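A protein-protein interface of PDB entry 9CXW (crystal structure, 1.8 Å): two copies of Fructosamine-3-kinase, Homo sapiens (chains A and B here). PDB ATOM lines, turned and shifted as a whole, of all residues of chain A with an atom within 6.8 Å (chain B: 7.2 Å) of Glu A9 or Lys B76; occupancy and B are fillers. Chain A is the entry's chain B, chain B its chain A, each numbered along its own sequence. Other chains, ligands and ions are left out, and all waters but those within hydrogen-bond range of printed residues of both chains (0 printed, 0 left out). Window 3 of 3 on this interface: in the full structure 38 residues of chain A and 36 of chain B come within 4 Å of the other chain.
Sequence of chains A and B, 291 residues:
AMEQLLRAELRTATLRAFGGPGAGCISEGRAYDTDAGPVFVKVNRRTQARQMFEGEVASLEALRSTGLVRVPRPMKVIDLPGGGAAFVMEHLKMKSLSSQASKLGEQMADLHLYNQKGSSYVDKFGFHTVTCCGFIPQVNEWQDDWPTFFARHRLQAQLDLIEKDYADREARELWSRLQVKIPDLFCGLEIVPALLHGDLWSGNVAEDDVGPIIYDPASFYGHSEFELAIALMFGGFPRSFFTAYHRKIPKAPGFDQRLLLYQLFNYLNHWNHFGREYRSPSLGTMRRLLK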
ATOM      1  N   GLN A   4      -7.329 -18.718 -26.242  1.00  0.00           N
ATOM      2  CA  GLN A   4      -8.108 -17.521 -26.548  1.00  0.00           C
ATOM      3  C   GLN A   4      -7.303 -16.263 -26.274  1.00  0.00           C
ATOM      4  O   GLN A   4      -7.303 -15.320 -27.076  1.00  0.00           O
ATOM      5  CB  GLN A   4      -9.406 -17.533 -25.744  1.00  0.00           C
ATOM      6  CG  GLN A   4     -10.299 -18.704 -26.149  1.00  0.00           C
ATOM      7  CD  GLN A   4     -10.673 -18.636 -27.629  1.00  0.00           C
ATOM      8  OE1 GLN A   4     -10.925 -17.550 -28.167  1.00  0.00           O
ATOM      9  NE2 GLN A   4     -10.702 -19.795 -28.297  1.00  0.00           N
ATOM     10  N   LEU A   5      -6.578 -16.251 -25.158  1.00  0.00           N
ATOM     11  CA  LEU A   5      -5.740 -15.101 -24.861  1.00  0.00           C
ATOM     12  C   LEU A   5      -4.669 -14.917 -25.930  1.00  0.00           C
ATOM     13  O   LEU A   5      -4.405 -13.789 -26.355  1.00  0.00           O
ATOM     14  CB  LEU A   5      -5.121 -15.260 -23.475  1.00  0.00           C
ATOM     15  CG  LEU A   5      -4.438 -14.018 -22.913  1.00  0.00           C
ATOM     16  CD1 LEU A   5      -5.475 -12.950 -22.556  1.00  0.00           C
ATOM     17  CD2 LEU A   5      -3.632 -14.433 -21.707  1.00  0.00           C
ATOM     18  N   LEU A   6      -4.066 -16.015 -26.401  1.00  0.00           N
ATOM     19  CA  LEU A   6      -3.021 -15.907 -27.423  1.00  0.00           C
ATOM     20  C   LEU A   6      -3.594 -15.398 -28.735  1.00  0.00           C
ATOM     21  O   LEU A   6      -3.022 -14.496 -29.350  1.00  0.00           O
ATOM     22  CB  LEU A   6      -2.312 -17.255 -27.622  1.00  0.00           C
ATOM     23  CG  LEU A   6      -1.415 -17.703 -26.455  1.00  0.00           C
ATOM     24  CD1 LEU A   6      -0.797 -19.064 -26.734  1.00  0.00           C
ATOM     25  CD2 LEU A   6      -0.317 -16.664 -26.184  1.00  0.00           C
ATOM     26  N   ARG A   7      -4.741 -15.950 -29.175  1.00  0.00           N
ATOM     27  CA  ARG A   7      -5.382 -15.452 -30.394  1.00  0.00           C
ATOM     28  C   ARG A   7      -5.635 -13.954 -30.305  1.00  0.00           C
ATOM     29  O   ARG A   7      -5.383 -13.218 -31.265  1.00  0.00           O
ATOM     30  CB  ARG A   7      -6.701 -16.186 -30.652  1.00  0.00           C
ATOM     31  CG  ARG A   7      -6.607 -17.706 -30.719  1.00  0.00           C
ATOM     32  CD  ARG A   7      -7.992 -18.326 -30.679  1.00  0.00           C
ATOM     33  NE  ARG A   7      -7.970 -19.784 -30.694  1.00  0.00           N
ATOM     34  CZ  ARG A   7      -7.986 -20.512 -31.803  1.00  0.00           C
ATOM     35  NH1 ARG A   7      -8.020 -19.942 -32.999  1.00  0.00           N
ATOM     36  NH2 ARG A   7      -7.953 -21.840 -31.711  1.00  0.00           N
ATOM     37  N   ALA A   8      -6.099 -13.476 -29.145  1.00  0.00           N
ATOM     38  CA  ALA A   8      -6.386 -12.046 -29.014  1.00  0.00           C
ATOM     39  C   ALA A   8      -5.113 -11.212 -28.939  1.00  0.00           C
ATOM     40  O   ALA A   8      -5.018 -10.143 -29.551  1.00  0.00           O
ATOM     41  CB  ALA A   8      -7.243 -11.795 -27.773  1.00  0.00           C
ATOM     42  N   GLU A   9      -4.149 -11.636 -28.122  1.00  0.00           N
ATOM     43  CA  GLU A   9      -2.957 -10.822 -27.927  1.00  0.00           C
ATOM     44  C   GLU A   9      -2.079 -10.791 -29.170  1.00  0.00           C
ATOM     45  O   GLU A   9      -1.410  -9.785 -29.422  1.00  0.00           O
ATOM     46  CB  GLU A   9      -2.171 -11.342 -26.731  1.00  0.00           C
ATOM     47  CG  GLU A   9      -2.877 -11.077 -25.421  1.00  0.00           C
ATOM     48  CD  GLU A   9      -2.564  -9.676 -24.930  1.00  0.00           C
ATOM     49  OE1 GLU A   9      -1.736  -9.004 -25.585  1.00  0.00           O
ATOM     50  OE2 GLU A   9      -3.144  -9.243 -23.913  1.00  0.00           O
ATOM     51  N   LEU A  10      -2.064 -11.884 -29.938  1.00  0.00           N
ATOM     52  CA  LEU A  10      -1.240 -12.015 -31.134  1.00  0.00           C
ATOM     53  C   LEU A  10      -1.985 -11.712 -32.427  1.00  0.00           C
ATOM     54  O   LEU A  10      -1.330 -11.455 -33.445  1.00  0.00           O
ATOM     55  CB  LEU A  10      -0.663 -13.434 -31.233  1.00  0.00           C
ATOM     56  CG  LEU A  10       0.338 -13.889 -30.164  1.00  0.00           C
ATOM     57  CD1 LEU A  10       0.874 -15.296 -30.483  1.00  0.00           C
ATOM     58  CD2 LEU A  10       1.464 -12.890 -29.930  1.00  0.00           C
ATOM     59  N   ARG A  11      -3.328 -11.707 -32.401  1.00  0.00           N
ATOM     60  CA  ARG A  11      -4.180 -11.361 -33.552  1.00  0.00           C
ATOM     61  C   ARG A  11      -4.138 -12.430 -34.649  1.00  0.00           C
ATOM     62  O   ARG A  11      -3.903 -12.130 -35.815  1.00  0.00           O
ATOM     63  CB  ARG A  11      -3.780  -9.990 -34.114  1.00  0.00           C
ATOM     64  CG  ARG A  11      -3.461  -8.967 -33.023  1.00  0.00           C
ATOM     65  CD  ARG A  11      -4.057  -7.604 -33.240  1.00  0.00           C
ATOM     66  NE  ARG A  11      -3.844  -6.761 -32.069  1.00  0.00           N
ATOM     67  CZ  ARG A  11      -2.900  -5.835 -31.966  1.00  0.00           C
ATOM     68  NH1 ARG A  11      -2.009  -5.648 -32.927  1.00  0.00           N
ATOM     69  NH2 ARG A  11      -2.850  -5.075 -30.871  1.00  0.00           N
ATOM     70  N   THR A  12      -4.411 -13.677 -34.278  1.00  0.00           N
ATOM     71  CA  THR A  12      -4.376 -14.798 -35.214  1.00  0.00           C
ATOM     72  C   THR A  12      -5.725 -15.514 -35.234  1.00  0.00           C
ATOM     73  O   THR A  12      -6.325 -15.770 -34.184  1.00  0.00           O
ATOM     74  CB  THR A  12      -3.227 -15.781 -34.850  1.00  0.00           C
ATOM     75  OG1 THR A  12      -3.331 -16.985 -35.622  1.00  0.00           O
ATOM     76  CG2 THR A  12      -3.240 -16.141 -33.354  1.00  0.00           C
ATOM     77  N   PHE B  40       6.727 -19.720 -30.281  1.00  0.00           N
ATOM     78  CA  PHE B  40       6.979 -20.569 -29.144  1.00  0.00           C
ATOM     79  C   PHE B  40       6.569 -19.796 -27.903  1.00  0.00           C
ATOM     80  O   PHE B  40       6.876 -18.609 -27.774  1.00  0.00           O
ATOM     81  CB  PHE B  40       8.451 -21.017 -29.094  1.00  0.00           C
ATOM     82  CG  PHE B  40       8.720 -22.031 -28.025  1.00  0.00           C
ATOM     83  CD1 PHE B  40       8.431 -23.379 -28.234  1.00  0.00           C
ATOM     84  CD2 PHE B  40       9.197 -21.641 -26.792  1.00  0.00           C
ATOM     85  CE1 PHE B  40       8.656 -24.316 -27.224  1.00  0.00           C
ATOM     86  CE2 PHE B  40       9.417 -22.575 -25.787  1.00  0.00           C
ATOM     87  CZ  PHE B  40       9.145 -23.903 -26.005  1.00  0.00           C
ATOM     88  N   LYS B  42       6.391 -19.662 -23.698  1.00  0.00           N
ATOM     89  CA  LYS B  42       6.813 -20.121 -22.383  1.00  0.00           C
ATOM     90  C   LYS B  42       5.806 -19.649 -21.358  1.00  0.00           C
ATOM     91  O   LYS B  42       5.442 -18.475 -21.347  1.00  0.00           O
ATOM     92  CB  LYS B  42       8.177 -19.542 -22.005  1.00  0.00           C
ATOM     93  CG  LYS B  42       9.338 -20.205 -22.595  1.00  0.00           C
ATOM     94  CD  LYS B  42      10.502 -19.703 -21.768  1.00  0.00           C
ATOM     95  CE  LYS B  42      11.767 -19.843 -22.482  1.00  0.00           C
ATOM     96  NZ  LYS B  42      12.888 -19.574 -21.536  1.00  0.00           N
ATOM     97  N   ARG B  50       6.346 -12.261 -14.732  1.00  0.00           N
ATOM     98  CA  ARG B  50       6.597 -11.116 -15.607  1.00  0.00           C
ATOM     99  C   ARG B  50       8.008 -10.574 -15.405  1.00  0.00           C
ATOM    100  O   ARG B  50       8.757 -10.393 -16.374  1.00  0.00           O
ATOM    101  CB  ARG B  50       5.586  -9.991 -15.370  1.00  0.00           C
ATOM    102  CG  ARG B  50       5.976  -8.718 -16.155  1.00  0.00           C
ATOM    103  CD  ARG B  50       4.855  -7.696 -16.282  1.00  0.00           C
ATOM    104  NE  ARG B  50       3.858  -8.033 -17.284  1.00  0.00           N
ATOM    105  CZ  ARG B  50       3.925  -7.741 -18.580  1.00  0.00           C
ATOM    106  NH1 ARG B  50       4.964  -7.115 -19.103  1.00  0.00           N
ATOM    107  NH2 ARG B  50       2.917  -8.095 -19.372  1.00  0.00           N
ATOM    108  N   PHE B  53      10.458 -12.854 -17.035  1.00  0.00           N
ATOM    109  CA  PHE B  53      10.458 -12.811 -18.479  1.00  0.00           C
ATOM    110  C   PHE B  53      10.982 -11.478 -18.962  1.00  0.00           C
ATOM    111  O   PHE B  53      11.659 -11.419 -20.000  1.00  0.00           O
ATOM    112  CB  PHE B  53       9.046 -13.079 -19.006  1.00  0.00           C
ATOM    113  CG  PHE B  53       8.638 -14.521 -18.921  1.00  0.00           C
ATOM    114  CD1 PHE B  53       9.538 -15.535 -19.237  1.00  0.00           C
ATOM    115  CD2 PHE B  53       7.330 -14.866 -18.553  1.00  0.00           C
ATOM    116  CE1 PHE B  53       9.153 -16.877 -19.189  1.00  0.00           C
ATOM    117  CE2 PHE B  53       6.930 -16.193 -18.510  1.00  0.00           C
ATOM    118  CZ  PHE B  53       7.834 -17.205 -18.840  1.00  0.00           C
ATOM    119  N   VAL B  57      13.788 -11.063 -21.721  1.00  0.00           N
ATOM    120  CA  VAL B  57      13.671 -10.219 -22.905  1.00  0.00           C
ATOM    121  C   VAL B  57      14.881  -9.296 -22.980  1.00  0.00           C
ATOM    122  O   VAL B  57      15.534  -9.189 -24.023  1.00  0.00           O
ATOM    123  CB  VAL B  57      12.358  -9.423 -22.893  1.00  0.00           C
ATOM    124  CG1 VAL B  57      12.432  -8.271 -23.918  1.00  0.00           C
ATOM    125  CG2 VAL B  57      11.161 -10.377 -23.191  1.00  0.00           C
ATOM    126  N   ARG B  73      13.782 -14.243 -31.342  1.00  0.00           N
ATOM    127  CA  ARG B  73      13.326 -12.865 -31.229  1.00  0.00           C
ATOM    128  C   ARG B  73      12.156 -12.785 -30.262  1.00  0.00           C
ATOM    129  O   ARG B  73      11.110 -13.399 -30.517  1.00  0.00           O
ATOM    130  CB  ARG B  73      12.885 -12.315 -32.588  1.00  0.00           C
ATOM    131  CG  ARG B  73      12.447 -10.830 -32.526  1.00  0.00           C
ATOM    132  CD  ARG B  73      12.148 -10.261 -33.923  1.00  0.00           C
ATOM    133  NE  ARG B  73      11.671  -8.878 -33.919  1.00  0.00           N
ATOM    134  CZ  ARG B  73      12.445  -7.808 -34.053  1.00  0.00           C
ATOM    135  NH1 ARG B  73      13.761  -7.910 -34.133  1.00  0.00           N
ATOM    136  NH2 ARG B  73      11.882  -6.604 -34.119  1.00  0.00           N
ATOM    137  N   PRO B  74      12.279 -12.041 -29.170  1.00  0.00           N
ATOM    138  CA  PRO B  74      11.151 -11.882 -28.246  1.00  0.00           C
ATOM    139  C   PRO B  74      10.006 -11.129 -28.905  1.00  0.00           C
ATOM    140  O   PRO B  74      10.216 -10.176 -29.666  1.00  0.00           O
ATOM    141  CB  PRO B  74      11.758 -11.081 -27.084  1.00  0.00           C
ATOM    142  CG  PRO B  74      12.955 -10.485 -27.586  1.00  0.00           C
ATOM    143  CD  PRO B  74      13.476 -11.304 -28.746  1.00  0.00           C
ATOM    144  N   MET B  75       8.781 -11.585 -28.649  1.00  0.00           N
ATOM    145  CA  MET B  75       7.611 -10.900 -29.193  1.00  0.00           C
ATOM    146  C   MET B  75       6.776 -10.210 -28.126  1.00  0.00           C
ATOM    147  O   MET B  75       6.546  -9.002 -28.218  1.00  0.00           O
ATOM    148  CB  MET B  75       6.723 -11.823 -30.042  1.00  0.00           C
ATOM    149  CG  MET B  75       7.411 -12.358 -31.280  1.00  0.00           C
ATOM    150  SD  MET B  75       6.653 -13.863 -31.877  1.00  0.00           S
ATOM    151  CE  MET B  75       5.252 -13.229 -32.843  1.00  0.00           C
ATOM    152  N   LYS B  76       6.323 -10.931 -27.107  1.00  0.00           N
ATOM    153  CA  LYS B  76       5.353 -10.319 -26.223  1.00  0.00           C
ATOM    154  C   LYS B  76       5.430 -10.993 -24.877  1.00  0.00           C
ATOM    155  O   LYS B  76       5.629 -12.205 -24.824  1.00  0.00           O
ATOM    156  CB  LYS B  76       3.926 -10.480 -26.776  1.00  0.00           C
ATOM    157  CG  LYS B  76       2.945  -9.362 -26.440  1.00  0.00           C
ATOM    158  CD  LYS B  76       1.659  -9.515 -27.265  1.00  0.00           C
ATOM    159  CE  LYS B  76       0.929  -8.174 -27.418  1.00  0.00           C
ATOM    160  NZ  LYS B  76       1.806  -7.052 -27.853  1.00  0.00           N
ATOM    161  N   VAL B  77       5.254 -10.216 -23.808  1.00  0.00           N
ATOM    162  CA  VAL B  77       5.017 -10.768 -22.471  1.00  0.00           C
ATOM    163  C   VAL B  77       3.582 -10.408 -22.064  1.00  0.00           C
ATOM    164  O   VAL B  77       3.225  -9.224 -21.973  1.00  0.00           O
ATOM    165  CB  VAL B  77       6.038 -10.254 -21.445  1.00  0.00           C
ATOM    166  CG1 VAL B  77       5.690 -10.752 -20.029  1.00  0.00           C
ATOM    167  CG2 VAL B  77       7.438 -10.724 -21.798  1.00  0.00           C
ATOM    168  N   ILE B  78       2.793 -11.430 -21.735  1.00  0.00           N
ATOM    169  CA  ILE B  78       1.352 -11.327 -21.517  1.00  0.00           C
ATOM    170  C   ILE B  78       1.032 -11.770 -20.096  1.00  0.00           C
ATOM    171  O   ILE B  78       1.429 -12.865 -19.683  1.00  0.00           O
ATOM    172  CB  ILE B  78       0.546 -12.183 -22.513  1.00  0.00           C
ATOM    173  CG1 ILE B  78       0.948 -11.912 -23.969  1.00  0.00           C
ATOM    174  CG2 ILE B  78      -0.959 -12.077 -22.262  1.00  0.00           C
ATOM    175  CD1 ILE B  78       0.611 -13.110 -24.888  1.00  0.00           C
ATOM    176  N   ASP B  79       0.289 -10.940 -19.367  1.00  0.00           N
ATOM    177  CA  ASP B  79      -0.145 -11.331 -18.028  1.00  0.00           C
ATOM    178  C   ASP B  79      -1.263 -12.374 -18.112  1.00  0.00           C
ATOM    179  O   ASP B  79      -2.177 -12.278 -18.941  1.00  0.00           O
ATOM    180  CB  ASP B  79      -0.591 -10.100 -17.247  1.00  0.00           C
ATOM    181  CG  ASP B  79       0.553  -9.124 -17.016  1.00  0.00           C
ATOM    182  OD1 ASP B  79       1.593  -9.528 -16.440  1.00  0.00           O
ATOM    183  OD2 ASP B  79       0.440  -7.957 -17.457  1.00  0.00           O
ATOM    184  N   ALA B  86       2.934 -15.283 -19.749  1.00  0.00           N
ATOM    185  CA  ALA B  86       3.315 -16.034 -20.929  1.00  0.00           C
ATOM    186  C   ALA B  86       4.304 -15.181 -21.709  1.00  0.00           C
ATOM    187  O   ALA B  86       4.136 -13.961 -21.810  1.00  0.00           O
ATOM    188  CB  ALA B  86       2.104 -16.354 -21.780  1.00  0.00           C
ATOM    189  N   PHE B  87       5.325 -15.816 -22.262  1.00  0.00           N
ATOM    190  CA  PHE B  87       6.344 -15.127 -23.052  1.00  0.00           C
ATOM    191  C   PHE B  87       6.325 -15.749 -24.429  1.00  0.00           C
ATOM    192  O   PHE B  87       6.618 -16.940 -24.575  1.00  0.00           O
ATOM    193  CB  PHE B  87       7.727 -15.237 -22.373  1.00  0.00           C
ATOM    194  CG  PHE B  87       8.892 -14.727 -23.212  1.00  0.00           C
ATOM    195  CD1 PHE B  87       8.746 -13.669 -24.089  1.00  0.00           C
ATOM    196  CD2 PHE B  87      10.135 -15.337 -23.109  1.00  0.00           C
ATOM    197  CE1 PHE B  87       9.818 -13.215 -24.855  1.00  0.00           C
ATOM    198  CE2 PHE B  87      11.241 -14.895 -23.867  1.00  0.00           C
ATOM    199  CZ  PHE B  87      11.082 -13.826 -24.750  1.00  0.00           C
ATOM    200  N   VAL B  88       5.948 -14.951 -25.432  1.00  0.00           N
ATOM    201  CA  VAL B  88       5.850 -15.390 -26.810  1.00  0.00           C
ATOM    202  C   VAL B  88       7.107 -14.934 -27.534  1.00  0.00           C
ATOM    203  O   VAL B  88       7.471 -13.744 -27.471  1.00  0.00           O
ATOM    204  CB  VAL B  88       4.598 -14.813 -27.484  1.00  0.00           C
ATOM    205  CG1 VAL B  88       4.411 -15.428 -28.858  1.00  0.00           C
ATOM    206  CG2 VAL B  88       3.388 -15.023 -26.617  1.00  0.00           C
ATOM    207  N   MET B  89       7.716 -15.859 -28.284  1.00  0.00           N
ATOM    208  CA  MET B  89       8.901 -15.537 -29.070  1.00  0.00           C
ATOM    209  C   MET B  89       8.815 -16.247 -30.414  1.00  0.00           C
ATOM    210  O   MET B  89       7.976 -17.124 -30.630  1.00  0.00           O
ATOM    211  CB  MET B  89      10.166 -15.906 -28.273  1.00  0.00           C
ATOM    212  CG  MET B  89      10.526 -17.370 -28.229  1.00  0.00           C
ATOM    213  SD  MET B  89      11.793 -17.706 -26.964  1.00  0.00           S
ATOM    214  CE  MET B  89      10.783 -17.905 -25.504  1.00  0.00           C
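Printed residues of chain B that touch a printed residue of chain A: Lys B76, Ile B78, Asp B79 and Val B88. Hydrophobic or aromatic side chains of chain B that line the printed part of chain A: Ile B78 and Val B88. Along chain B the printed residues that touch a printed residue of chain A span positions 76 to 88. Printed residues of chain A that touch a printed residue of chain B: Leu A5, Leu A6, Glu A9 and Leu A10. Hydrophobic or aromatic side chains of chain A that line the printed part of chain B: Leu A5, Leu A6 and Leu A10. Among the printed residues, 6 pairs touch across the chains. Among the printed residues, no Asp or Glu carboxylate lies within 4 Å of a Lys or Arg side-chain nitrogen of the other chain.
Leu A5 touches Ile B78 (CD2 to CG2, 3.6 Å). Leu A5 touches Asp B79 (CD2 to O, 3.8 Å). Leu A6 touches Ile B78 (CD2 to CD1, 3.9 Å). Lys B76 touches Glu A9. CB of Glu A9 touches CD1 of Ile B78, 3.8 Å away. CD1 of Leu A10 touches CG1 of Val B88, at 3.9 Å.
Glu A9 touches two residues of chain B. Of the printed residues of chain A, Lys B76 touches Glu A9 (3.3 Å). Printed residues of chain A within 4 Å of Ile B78: Leu A5, Leu A6 and Glu A9. Printed residues of chain A within 4 Å of Asp B79: Leu A5. Met B89 touches none of the printed residues of chain A. The nearest residue of chain B that does not touch Glu A9 is Asp B79 (5.9 Å).
No position is printed for both chains. Of the 6 pairs that touch across the chains among the printed residues, none has its exchanged pair printed and touching as well.
The backbone NH (N) of Val B88 is in hydrogen-bond range of the backbone carbonyl oxygen (O) of Lys B76 (2.8 Å). The backbone NH of Met B75 lies within hydrogen-bond range of the backbone carbonyl oxygen of Val B88 (2.8 Å). The guanidinium group of Arg B50 lies within salt-bridge range of the side-chain carboxylate of Asp B79, at 2.8 Å. The backbone carbonyl oxygen of Ile B78 lies within hydrogen-bond range of the backbone NH of Ala B86 (2.8 Å).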
